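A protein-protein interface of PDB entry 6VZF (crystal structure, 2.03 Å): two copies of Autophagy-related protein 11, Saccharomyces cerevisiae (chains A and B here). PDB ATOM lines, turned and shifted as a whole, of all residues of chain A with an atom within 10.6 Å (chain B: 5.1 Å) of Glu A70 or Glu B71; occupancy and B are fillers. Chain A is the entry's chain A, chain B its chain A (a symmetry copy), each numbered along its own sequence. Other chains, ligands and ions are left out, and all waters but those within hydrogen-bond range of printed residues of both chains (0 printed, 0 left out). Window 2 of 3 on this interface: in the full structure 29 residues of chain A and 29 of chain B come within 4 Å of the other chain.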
ATOM      1  N   GLN A  62      -9.005 -29.067 -15.978  1.00  0.00           N
ATOM      2  CA  GLN A  62     -10.256 -29.451 -16.664  1.00  0.00           C
ATOM      3  C   GLN A  62     -11.246 -28.281 -16.668  1.00  0.00           C
ATOM      4  O   GLN A  62     -11.656 -27.934 -17.743  1.00  0.00           O
ATOM      5  CB  GLN A  62     -10.840 -30.715 -16.047  1.00  0.00           C
ATOM      6  CG  GLN A  62     -10.146 -31.966 -16.549  1.00  0.00           C
ATOM      7  CD  GLN A  62     -10.723 -33.230 -15.941  1.00  0.00           C
ATOM      8  OE1 GLN A  62      -9.998 -34.182 -15.632  1.00  0.00           O
ATOM      9  NE2 GLN A  62     -12.037 -33.249 -15.759  1.00  0.00           N
ATOM     10  N   GLU A  63     -11.510 -27.627 -15.537  1.00  0.00           N
ATOM     11  CA  GLU A  63     -12.412 -26.455 -15.472  1.00  0.00           C
ATOM     12  C   GLU A  63     -11.848 -25.354 -16.337  1.00  0.00           C
ATOM     13  O   GLU A  63     -12.619 -24.672 -17.016  1.00  0.00           O
ATOM     14  CB  GLU A  63     -12.617 -25.914 -14.069  1.00  0.00           C
ATOM     15  CG  GLU A  63     -13.062 -27.011 -13.130  1.00  0.00           C
ATOM     16  CD  GLU A  63     -13.527 -26.558 -11.758  1.00  0.00           C
ATOM     17  OE1 GLU A  63     -13.651 -25.316 -11.544  1.00  0.00           O
ATOM     18  OE2 GLU A  63     -13.787 -27.457 -10.913  1.00  0.00           O
ATOM     19  N   LEU A  64     -10.549 -25.138 -16.254  1.00  0.00           N
ATOM     20  CA  LEU A  64      -9.893 -24.061 -17.027  1.00  0.00           C
ATOM     21  C   LEU A  64     -10.083 -24.286 -18.530  1.00  0.00           C
ATOM     22  O   LEU A  64     -10.433 -23.280 -19.212  1.00  0.00           O
ATOM     23  CB  LEU A  64      -8.418 -23.973 -16.667  1.00  0.00           C
ATOM     24  CG  LEU A  64      -7.654 -22.808 -17.286  1.00  0.00           C
ATOM     25  CD1 LEU A  64      -8.372 -21.498 -17.039  1.00  0.00           C
ATOM     26  CD2 LEU A  64      -6.256 -22.751 -16.692  1.00  0.00           C
ATOM     27  N   ALA A  65      -9.844 -25.502 -19.020  1.00  0.00           N
ATOM     28  CA  ALA A  65     -10.077 -25.906 -20.425  1.00  0.00           C
ATOM     29  C   ALA A  65     -11.535 -25.616 -20.808  1.00  0.00           C
ATOM     30  O   ALA A  65     -11.773 -25.167 -21.923  1.00  0.00           O
ATOM     31  CB  ALA A  65      -9.849 -27.379 -20.617  1.00  0.00           C
ATOM     32  N   ARG A  66     -12.461 -25.993 -19.934  1.00  0.00           N
ATOM     33  CA  ARG A  66     -13.914 -25.901 -20.154  1.00  0.00           C
ATOM     34  C   ARG A  66     -14.247 -24.414 -20.337  1.00  0.00           C
ATOM     35  O   ARG A  66     -14.744 -24.062 -21.426  1.00  0.00           O
ATOM     36  CB  ARG A  66     -14.628 -26.624 -19.017  1.00  0.00           C
ATOM     37  CG  ARG A  66     -15.884 -27.353 -19.454  1.00  0.00           C
ATOM     38  CD  ARG A  66     -16.923 -27.543 -18.362  1.00  0.00           C
ATOM     39  NE  ARG A  66     -17.175 -26.433 -17.441  1.00  0.00           N
ATOM     40  CZ  ARG A  66     -17.265 -25.126 -17.739  1.00  0.00           C
ATOM     41  NH1 ARG A  66     -17.147 -24.675 -18.979  1.00  0.00           N
ATOM     42  NH2 ARG A  66     -17.490 -24.257 -16.764  1.00  0.00           N
ATOM     43  N   LEU A  67     -13.887 -23.560 -19.373  1.00  0.00           N
ATOM     44  CA  LEU A  67     -14.101 -22.099 -19.469  1.00  0.00           C
ATOM     45  C   LEU A  67     -13.478 -21.542 -20.740  1.00  0.00           C
ATOM     46  O   LEU A  67     -14.172 -20.749 -21.405  1.00  0.00           O
ATOM     47  CB  LEU A  67     -13.516 -21.327 -18.293  1.00  0.00           C
ATOM     48  CG  LEU A  67     -14.336 -21.310 -17.015  1.00  0.00           C
ATOM     49  CD1 LEU A  67     -14.236 -19.959 -16.344  1.00  0.00           C
ATOM     50  CD2 LEU A  67     -15.781 -21.677 -17.281  1.00  0.00           C
ATOM     51  N   THR A  68     -12.198 -21.803 -21.007  1.00  0.00           N
ATOM     52  CA  THR A  68     -11.502 -21.058 -22.083  1.00  0.00           C
ATOM     53  C   THR A  68     -12.158 -21.421 -23.417  1.00  0.00           C
ATOM     54  O   THR A  68     -12.201 -20.550 -24.293  1.00  0.00           O
ATOM     55  CB  THR A  68      -9.993 -21.284 -22.210  1.00  0.00           C
ATOM     56  OG1 THR A  68      -9.913 -22.512 -22.922  1.00  0.00           O
ATOM     57  CG2 THR A  68      -9.219 -21.259 -20.908  1.00  0.00           C
ATOM     58  N   ASN A  69     -12.618 -22.666 -23.545  1.00  0.00           N
ATOM     59  CA  ASN A  69     -13.317 -23.202 -24.740  1.00  0.00           C
ATOM     60  C   ASN A  69     -14.631 -22.423 -24.920  1.00  0.00           C
ATOM     61  O   ASN A  69     -14.956 -22.092 -26.073  1.00  0.00           O
ATOM     62  CB  ASN A  69     -13.538 -24.711 -24.623  1.00  0.00           C
ATOM     63  CG  ASN A  69     -14.284 -25.305 -25.798  1.00  0.00           C
ATOM     64  OD1 ASN A  69     -13.678 -25.862 -26.709  1.00  0.00           O
ATOM     65  ND2 ASN A  69     -15.603 -25.194 -25.789  1.00  0.00           N
ATOM     66  N   GLU A  70     -15.337 -22.131 -23.820  1.00  0.00           N
ATOM     67  CA  GLU A  70     -16.592 -21.337 -23.813  1.00  0.00           C
ATOM     68  C   GLU A  70     -16.304 -19.882 -24.171  1.00  0.00           C
ATOM     69  O   GLU A  70     -16.811 -19.428 -25.204  1.00  0.00           O
ATOM     70  CB  GLU A  70     -17.270 -21.345 -22.452  1.00  0.00           C
ATOM     71  CG  GLU A  70     -18.139 -22.562 -22.241  1.00  0.00           C
ATOM     72  CD  GLU A  70     -19.121 -22.375 -21.101  1.00  0.00           C
ATOM     73  OE1 GLU A  70     -19.763 -21.296 -21.044  1.00  0.00           O
ATOM     74  OE2 GLU A  70     -19.232 -23.300 -20.268  1.00  0.00           O
ATOM     75  N   GLU A  71     -15.564 -19.169 -23.325  1.00  0.00           N
ATOM     76  CA  GLU A  71     -15.086 -17.794 -23.610  1.00  0.00           C
ATOM     77  C   GLU A  71     -14.648 -17.676 -25.075  1.00  0.00           C
ATOM     78  O   GLU A  71     -14.731 -16.558 -25.604  1.00  0.00           O
ATOM     79  CB  GLU A  71     -13.890 -17.436 -22.733  1.00  0.00           C
ATOM     80  CG  GLU A  71     -13.406 -15.998 -22.878  1.00  0.00           C
ATOM     81  CD  GLU A  71     -13.641 -15.115 -21.662  1.00  0.00           C
ATOM     82  OE1 GLU A  71     -12.736 -14.316 -21.344  1.00  0.00           O
ATOM     83  OE2 GLU A  71     -14.720 -15.228 -21.020  1.00  0.00           O
ATOM     84  N   GLN A  72     -14.147 -18.748 -25.701  1.00  0.00           N
ATOM     85  CA  GLN A  72     -13.658 -18.671 -27.104  1.00  0.00           C
ATOM     86  C   GLN A  72     -14.847 -18.749 -28.068  1.00  0.00           C
ATOM     87  O   GLN A  72     -14.946 -17.857 -28.915  1.00  0.00           O
ATOM     88  CB  GLN A  72     -12.632 -19.751 -27.446  1.00  0.00           C
ATOM     89  CG  GLN A  72     -11.765 -19.403 -28.654  1.00  0.00           C
ATOM     90  CD  GLN A  72     -11.420 -17.934 -28.748  1.00  0.00           C
ATOM     91  OE1 GLN A  72     -12.182 -17.123 -29.273  1.00  0.00           O
ATOM     92  NE2 GLN A  72     -10.251 -17.573 -28.249  1.00  0.00           N
ATOM     93  N   SER A  73     -15.691 -19.780 -27.957  1.00  0.00           N
ATOM     94  CA  SER A  73     -16.876 -20.001 -28.826  1.00  0.00           C
ATOM     95  C   SER A  73     -17.830 -18.798 -28.705  1.00  0.00           C
ATOM     96  O   SER A  73     -18.416 -18.414 -29.728  1.00  0.00           O
ATOM     97  CB  SER A  73     -17.562 -21.315 -28.515  1.00  0.00           C
ATOM     98  OG  SER A  73     -18.186 -21.274 -27.241  1.00  0.00           O
ATOM     99  N   HIS A  74     -17.938 -18.198 -27.514  1.00  0.00           N
ATOM    100  CA  HIS A  74     -18.766 -16.995 -27.227  1.00  0.00           C
ATOM    101  C   HIS A  74     -18.144 -15.762 -27.890  1.00  0.00           C
ATOM    102  O   HIS A  74     -18.896 -15.006 -28.530  1.00  0.00           O
ATOM    103  CB  HIS A  74     -18.941 -16.780 -25.721  1.00  0.00           C
ATOM    104  CG  HIS A  74     -19.934 -17.698 -25.088  1.00  0.00           C
ATOM    105  ND1 HIS A  74     -20.367 -17.525 -23.787  1.00  0.00           N
ATOM    106  CD2 HIS A  74     -20.595 -18.775 -25.566  1.00  0.00           C
ATOM    107  CE1 HIS A  74     -21.242 -18.465 -23.482  1.00  0.00           C
ATOM    108  NE2 HIS A  74     -21.402 -19.246 -24.559  1.00  0.00           N
ATOM    109  N   ARG A  75     -16.833 -15.571 -27.738  1.00  0.00           N
ATOM    110  CA  ARG A  75     -16.061 -14.466 -28.370  1.00  0.00           C
ATOM    111  C   ARG A  75     -16.194 -14.525 -29.900  1.00  0.00           C
ATOM    112  O   ARG A  75     -16.368 -13.443 -30.503  1.00  0.00           O
ATOM    113  CB  ARG A  75     -14.583 -14.555 -27.985  1.00  0.00           C
ATOM    114  CG  ARG A  75     -13.758 -13.334 -28.360  1.00  0.00           C
ATOM    115  CD  ARG A  75     -12.362 -13.442 -27.772  1.00  0.00           C
ATOM    116  NE  ARG A  75     -12.019 -12.306 -26.927  1.00  0.00           N
ATOM    117  CZ  ARG A  75     -12.615 -11.989 -25.771  1.00  0.00           C
ATOM    118  NH1 ARG A  75     -13.620 -12.712 -25.299  1.00  0.00           N
ATOM    119  NH2 ARG A  75     -12.209 -10.929 -25.091  1.00  0.00           N
ATOM    120  N   THR A  76     -16.080 -15.722 -30.499  1.00  0.00           N
ATOM    121  CA  THR A  76     -16.196 -15.954 -31.969  1.00  0.00           C
ATOM    122  C   THR A  76     -17.607 -15.568 -32.426  1.00  0.00           C
ATOM    123  O   THR A  76     -17.717 -14.689 -33.296  1.00  0.00           O
ATOM    124  CB  THR A  76     -15.923 -17.405 -32.401  1.00  0.00           C
ATOM    125  OG1 THR A  76     -16.910 -18.273 -31.838  1.00  0.00           O
ATOM    126  CG2 THR A  76     -14.540 -17.897 -32.032  1.00  0.00           C
ATOM    127  N   GLU A  77     -18.629 -16.197 -31.837  1.00  0.00           N
ATOM    128  CA  GLU A  77     -20.064 -16.027 -32.194  1.00  0.00           C
ATOM    129  C   GLU A  77     -20.446 -14.537 -32.189  1.00  0.00           C
ATOM    130  O   GLU A  77     -21.223 -14.145 -33.079  1.00  0.00           O
ATOM    131  CB  GLU A  77     -20.950 -16.828 -31.236  1.00  0.00           C
ATOM    132  CG  GLU A  77     -20.849 -18.336 -31.405  1.00  0.00           C
ATOM    133  CD  GLU A  77     -21.327 -19.159 -30.215  1.00  0.00           C
ATOM    134  OE1 GLU A  77     -21.256 -18.661 -29.069  1.00  0.00           O
ATOM    135  OE2 GLU A  77     -21.770 -20.305 -30.433  1.00  0.00           O
ATOM    136  N   ILE A  78     -19.916 -13.742 -31.246  1.00  0.00           N
ATOM    137  CA  ILE A  78     -20.243 -12.290 -31.059  1.00  0.00           C
ATOM    138  C   ILE A  78     -19.506 -11.440 -32.104  1.00  0.00           C
ATOM    139  O   ILE A  78     -19.979 -10.317 -32.394  1.00  0.00           O
ATOM    140  CB  ILE A  78     -19.941 -11.816 -29.619  1.00  0.00           C
ATOM    141  CG1 ILE A  78     -21.137 -12.040 -28.689  1.00  0.00           C
ATOM    142  CG2 ILE A  78     -19.494 -10.366 -29.585  1.00  0.00           C
ATOM    143  CD1 ILE A  78     -21.099 -11.221 -27.416  1.00  0.00           C
ATOM    144  N   LEU B  67     -10.585 -15.664 -15.657  1.00  0.00           N
ATOM    145  CA  LEU B  67     -11.621 -16.106 -16.616  1.00  0.00           C
ATOM    146  C   LEU B  67     -13.005 -16.043 -15.987  1.00  0.00           C
ATOM    147  O   LEU B  67     -13.911 -15.531 -16.672  1.00  0.00           O
ATOM    148  CB  LEU B  67     -11.409 -17.529 -17.119  1.00  0.00           C
ATOM    149  CG  LEU B  67     -10.383 -17.714 -18.223  1.00  0.00           C
ATOM    150  CD1 LEU B  67     -10.850 -18.765 -19.204  1.00  0.00           C
ATOM    151  CD2 LEU B  67     -10.091 -16.406 -18.930  1.00  0.00           C
ATOM    152  N   THR B  68     -13.218 -16.651 -14.819  1.00  0.00           N
ATOM    153  CA  THR B  68     -14.605 -16.834 -14.326  1.00  0.00           C
ATOM    154  C   THR B  68     -15.198 -15.452 -14.047  1.00  0.00           C
ATOM    155  O   THR B  68     -16.411 -15.299 -14.230  1.00  0.00           O
ATOM    156  CB  THR B  68     -14.779 -17.696 -13.072  1.00  0.00           C
ATOM    157  OG1 THR B  68     -14.454 -16.798 -12.019  1.00  0.00           O
ATOM    158  CG2 THR B  68     -13.994 -18.992 -13.059  1.00  0.00           C
ATOM    159  N   ASN B  69     -14.362 -14.514 -13.601  1.00  0.00           N
ATOM    160  CA  ASN B  69     -14.731 -13.106 -13.308  1.00  0.00           C
ATOM    161  C   ASN B  69     -15.186 -12.443 -14.620  1.00  0.00           C
ATOM    162  O   ASN B  69     -16.179 -11.698 -14.581  1.00  0.00           O
ATOM    163  CB  ASN B  69     -13.578 -12.357 -12.638  1.00  0.00           C
ATOM    164  CG  ASN B  69     -13.886 -10.903 -12.353  1.00  0.00           C
ATOM    165  OD1 ASN B  69     -14.248 -10.546 -11.235  1.00  0.00           O
ATOM    166  ND2 ASN B  69     -13.748 -10.052 -13.358  1.00  0.00           N
ATOM    167  N   GLU B  70     -14.493 -12.725 -15.731  1.00  0.00           N
ATOM    168  CA  GLU B  70     -14.833 -12.217 -17.085  1.00  0.00           C
ATOM    169  C   GLU B  70     -16.132 -12.849 -17.580  1.00  0.00           C
ATOM    170  O   GLU B  70     -17.096 -12.103 -17.788  1.00  0.00           O
ATOM    171  CB  GLU B  70     -13.754 -12.536 -18.107  1.00  0.00           C
ATOM    172  CG  GLU B  70     -12.632 -11.526 -18.104  1.00  0.00           C
ATOM    173  CD  GLU B  70     -11.794 -11.595 -19.367  1.00  0.00           C
ATOM    174  OE1 GLU B  70     -12.392 -11.663 -20.470  1.00  0.00           O
ATOM    175  OE2 GLU B  70     -10.551 -11.594 -19.244  1.00  0.00           O
ATOM    176  N   GLU B  71     -16.138 -14.160 -17.806  1.00  0.00           N
ATOM    177  CA  GLU B  71     -17.359 -14.929 -18.148  1.00  0.00           C
ATOM    178  C   GLU B  71     -18.549 -14.433 -17.318  1.00  0.00           C
ATOM    179  O   GLU B  71     -19.679 -14.562 -17.813  1.00  0.00           O
ATOM    180  CB  GLU B  71     -17.172 -16.415 -17.858  1.00  0.00           C
ATOM    181  CG  GLU B  71     -18.338 -17.297 -18.289  1.00  0.00           C
ATOM    182  CD  GLU B  71     -18.042 -18.229 -19.454  1.00  0.00           C
ATOM    183  OE1 GLU B  71     -18.509 -19.386 -19.401  1.00  0.00           O
ATOM    184  OE2 GLU B  71     -17.338 -17.810 -20.412  1.00  0.00           O
ATOM    185  N   GLN B  72     -18.338 -13.942 -16.091  1.00  0.00           N
ATOM    186  CA  GLN B  72     -19.465 -13.499 -15.226  1.00  0.00           C
ATOM    187  C   GLN B  72     -19.907 -12.091 -15.639  1.00  0.00           C
ATOM    188  O   GLN B  72     -21.104 -11.925 -15.886  1.00  0.00           O
ATOM    189  CB  GLN B  72     -19.129 -13.530 -13.735  1.00  0.00           C
ATOM    190  CG  GLN B  72     -20.363 -13.578 -12.837  1.00  0.00           C
ATOM    191  CD  GLN B  72     -21.492 -14.408 -13.404  1.00  0.00           C
ATOM    192  OE1 GLN B  72     -22.301 -13.939 -14.205  1.00  0.00           O
ATOM    193  NE2 GLN B  72     -21.571 -15.658 -12.984  1.00  0.00           N
ATOM    194  N   SER B  73     -18.987 -11.122 -15.685  1.00  0.00           N
ATOM    195  CA  SER B  73     -19.264  -9.708 -16.050  1.00  0.00           C
ATOM    196  C   SER B  73     -19.852  -9.654 -17.473  1.00  0.00           C
ATOM    197  O   SER B  73     -20.749  -8.829 -17.701  1.00  0.00           O
ATOM    198  CB  SER B  73     -18.033  -8.839 -15.902  1.00  0.00           C
ATOM    199  OG  SER B  73     -17.058  -9.166 -16.879  1.00  0.00           O
ATOM    200  N   HIS B  74     -19.401 -10.535 -18.375  1.00  0.00           N
ATOM    201  CA  HIS B  74     -19.892 -10.662 -19.773  1.00  0.00           C
ATOM    202  C   HIS B  74     -21.307 -11.248 -19.780  1.00  0.00           C
ATOM    203  O   HIS B  74     -22.161 -10.695 -20.496  1.00  0.00           O
ATOM    204  CB  HIS B  74     -18.942 -11.509 -20.626  1.00  0.00           C
ATOM    205  CG  HIS B  74     -17.705 -10.790 -21.053  1.00  0.00           C
ATOM    206  ND1 HIS B  74     -16.831 -11.322 -21.982  1.00  0.00           N
ATOM    207  CD2 HIS B  74     -17.201  -9.585 -20.707  1.00  0.00           C
ATOM    208  CE1 HIS B  74     -15.831 -10.484 -22.181  1.00  0.00           C
ATOM    209  NE2 HIS B  74     -16.035  -9.407 -21.412  1.00  0.00           N
ATOM    210  N   ARG B  75     -21.538 -12.319 -19.021  1.00  0.00           N
ATOM    211  CA  ARG B  75     -22.867 -12.970 -18.859  1.00  0.00           C
ATOM    212  C   ARG B  75     -23.892 -11.968 -18.306  1.00  0.00           C
ATOM    213  O   ARG B  75     -25.035 -11.975 -18.815  1.00  0.00           O
ATOM    214  CB  ARG B  75     -22.767 -14.168 -17.913  1.00  0.00           C
ATOM    215  CG  ARG B  75     -24.002 -15.054 -17.884  1.00  0.00           C
ATOM    216  CD  ARG B  75     -23.732 -16.305 -17.065  1.00  0.00           C
ATOM    217  NE  ARG B  75     -23.966 -17.531 -17.819  1.00  0.00           N
ATOM    218  CZ  ARG B  75     -23.268 -17.930 -18.889  1.00  0.00           C
ATOM    219  NH1 ARG B  75     -22.278 -17.196 -19.373  1.00  0.00           N
ATOM    220  NH2 ARG B  75     -23.577 -19.070 -19.487  1.00  0.00           N
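The side-chain carboxylate of Glu B71 sits close to the side-chain carboxylate of Glu A70. OE1 of Glu A71 lies close to OE1 of Glu B70 (2.8 Å).
O of Ala A65 is in hydrogen-bond range of OG1 of Thr A68, at 3.4 Å. NH1 of Arg A66 is in salt-bridge range of OE2 of Glu A70, at 2.8 Å. O of Glu A70 sits at hydrogen-bond distance from OG of Ser A73. The backbone carbonyl oxygen (O) of Glu B70 lies within hydrogen-bond range of the side-chain hydroxyl (OG) of Ser B73, at 3.1 Å.
Among the printed residues, pairs that only touch across the chains: Thr A68 with Leu B67 (3.4 Å), Leu A67 with Thr B68 (3.4 Å), Glu A71 with Glu B71 (3.7 Å) and Leu A67 with Leu B67 (3.8 Å).
Gln A62 touches none of the printed residues of chain B. Ala A65 touches none of the printed residues of chain B. Of the printed residues of chain B, Leu A67 touches Leu B67 and Thr B68. Of chain B, only Glu B71 (2.8 Å) comes within 4 Å of Glu A70. Of the printed residues of chain B, Glu A71 touches Glu B70 (2.8 Å) and Glu B71 (3.7 Å). Of the printed residues of chain A, Leu B67 touches Leu A67 and Thr A68. Printed residues of chain A within 4 Å of Thr B68: Leu A67 (3.4 Å). Glu B70 touches just one residue of chain A: Glu A71 (2.8 Å). Of chain A, only Glu A70 (2.8 Å) and Glu A71 (3.7 Å) come within 4 Å of Glu B71. No residue of chain A comes within 4 Å of His B74. Arg B75 touches none of the printed residues of chain A. The nearest residue of chain B that does not touch Glu A70 is Arg B75 (4.7 Å). The nearest residue of chain A that does not touch Glu B71 is Leu A67 (4.1 Å).
Of the 17 printed residues of chain A, 4 touch a printed residue of chain B. Hydrophobic or aromatic side chains of chain A that line the printed part of chain B: Leu A67. Of the 9 printed residues of chain B, 4 touch a printed residue of chain A. Hydrophobic or aromatic side chains of chain B that line the printed part of chain A: Leu B67. Along chain B the printed residues that touch a printed residue of chain A span positions 67 to 71. Among the printed residues, 6 pairs touch across the chains. Among the printed residues, no Asp or Glu carboxylate lies within 4 Å of a Lys or Arg side-chain nitrogen of the other chain.
Leu A67 touches its own counterpart, Leu B67. Leu A67 touches Thr B68, and with the chains exchanged Thr A68 touches Leu B67. Glu A70 touches Glu B71, and with the chains exchanged Glu A71 touches Glu B70. Glu A71 touches its own counterpart, Glu B71.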
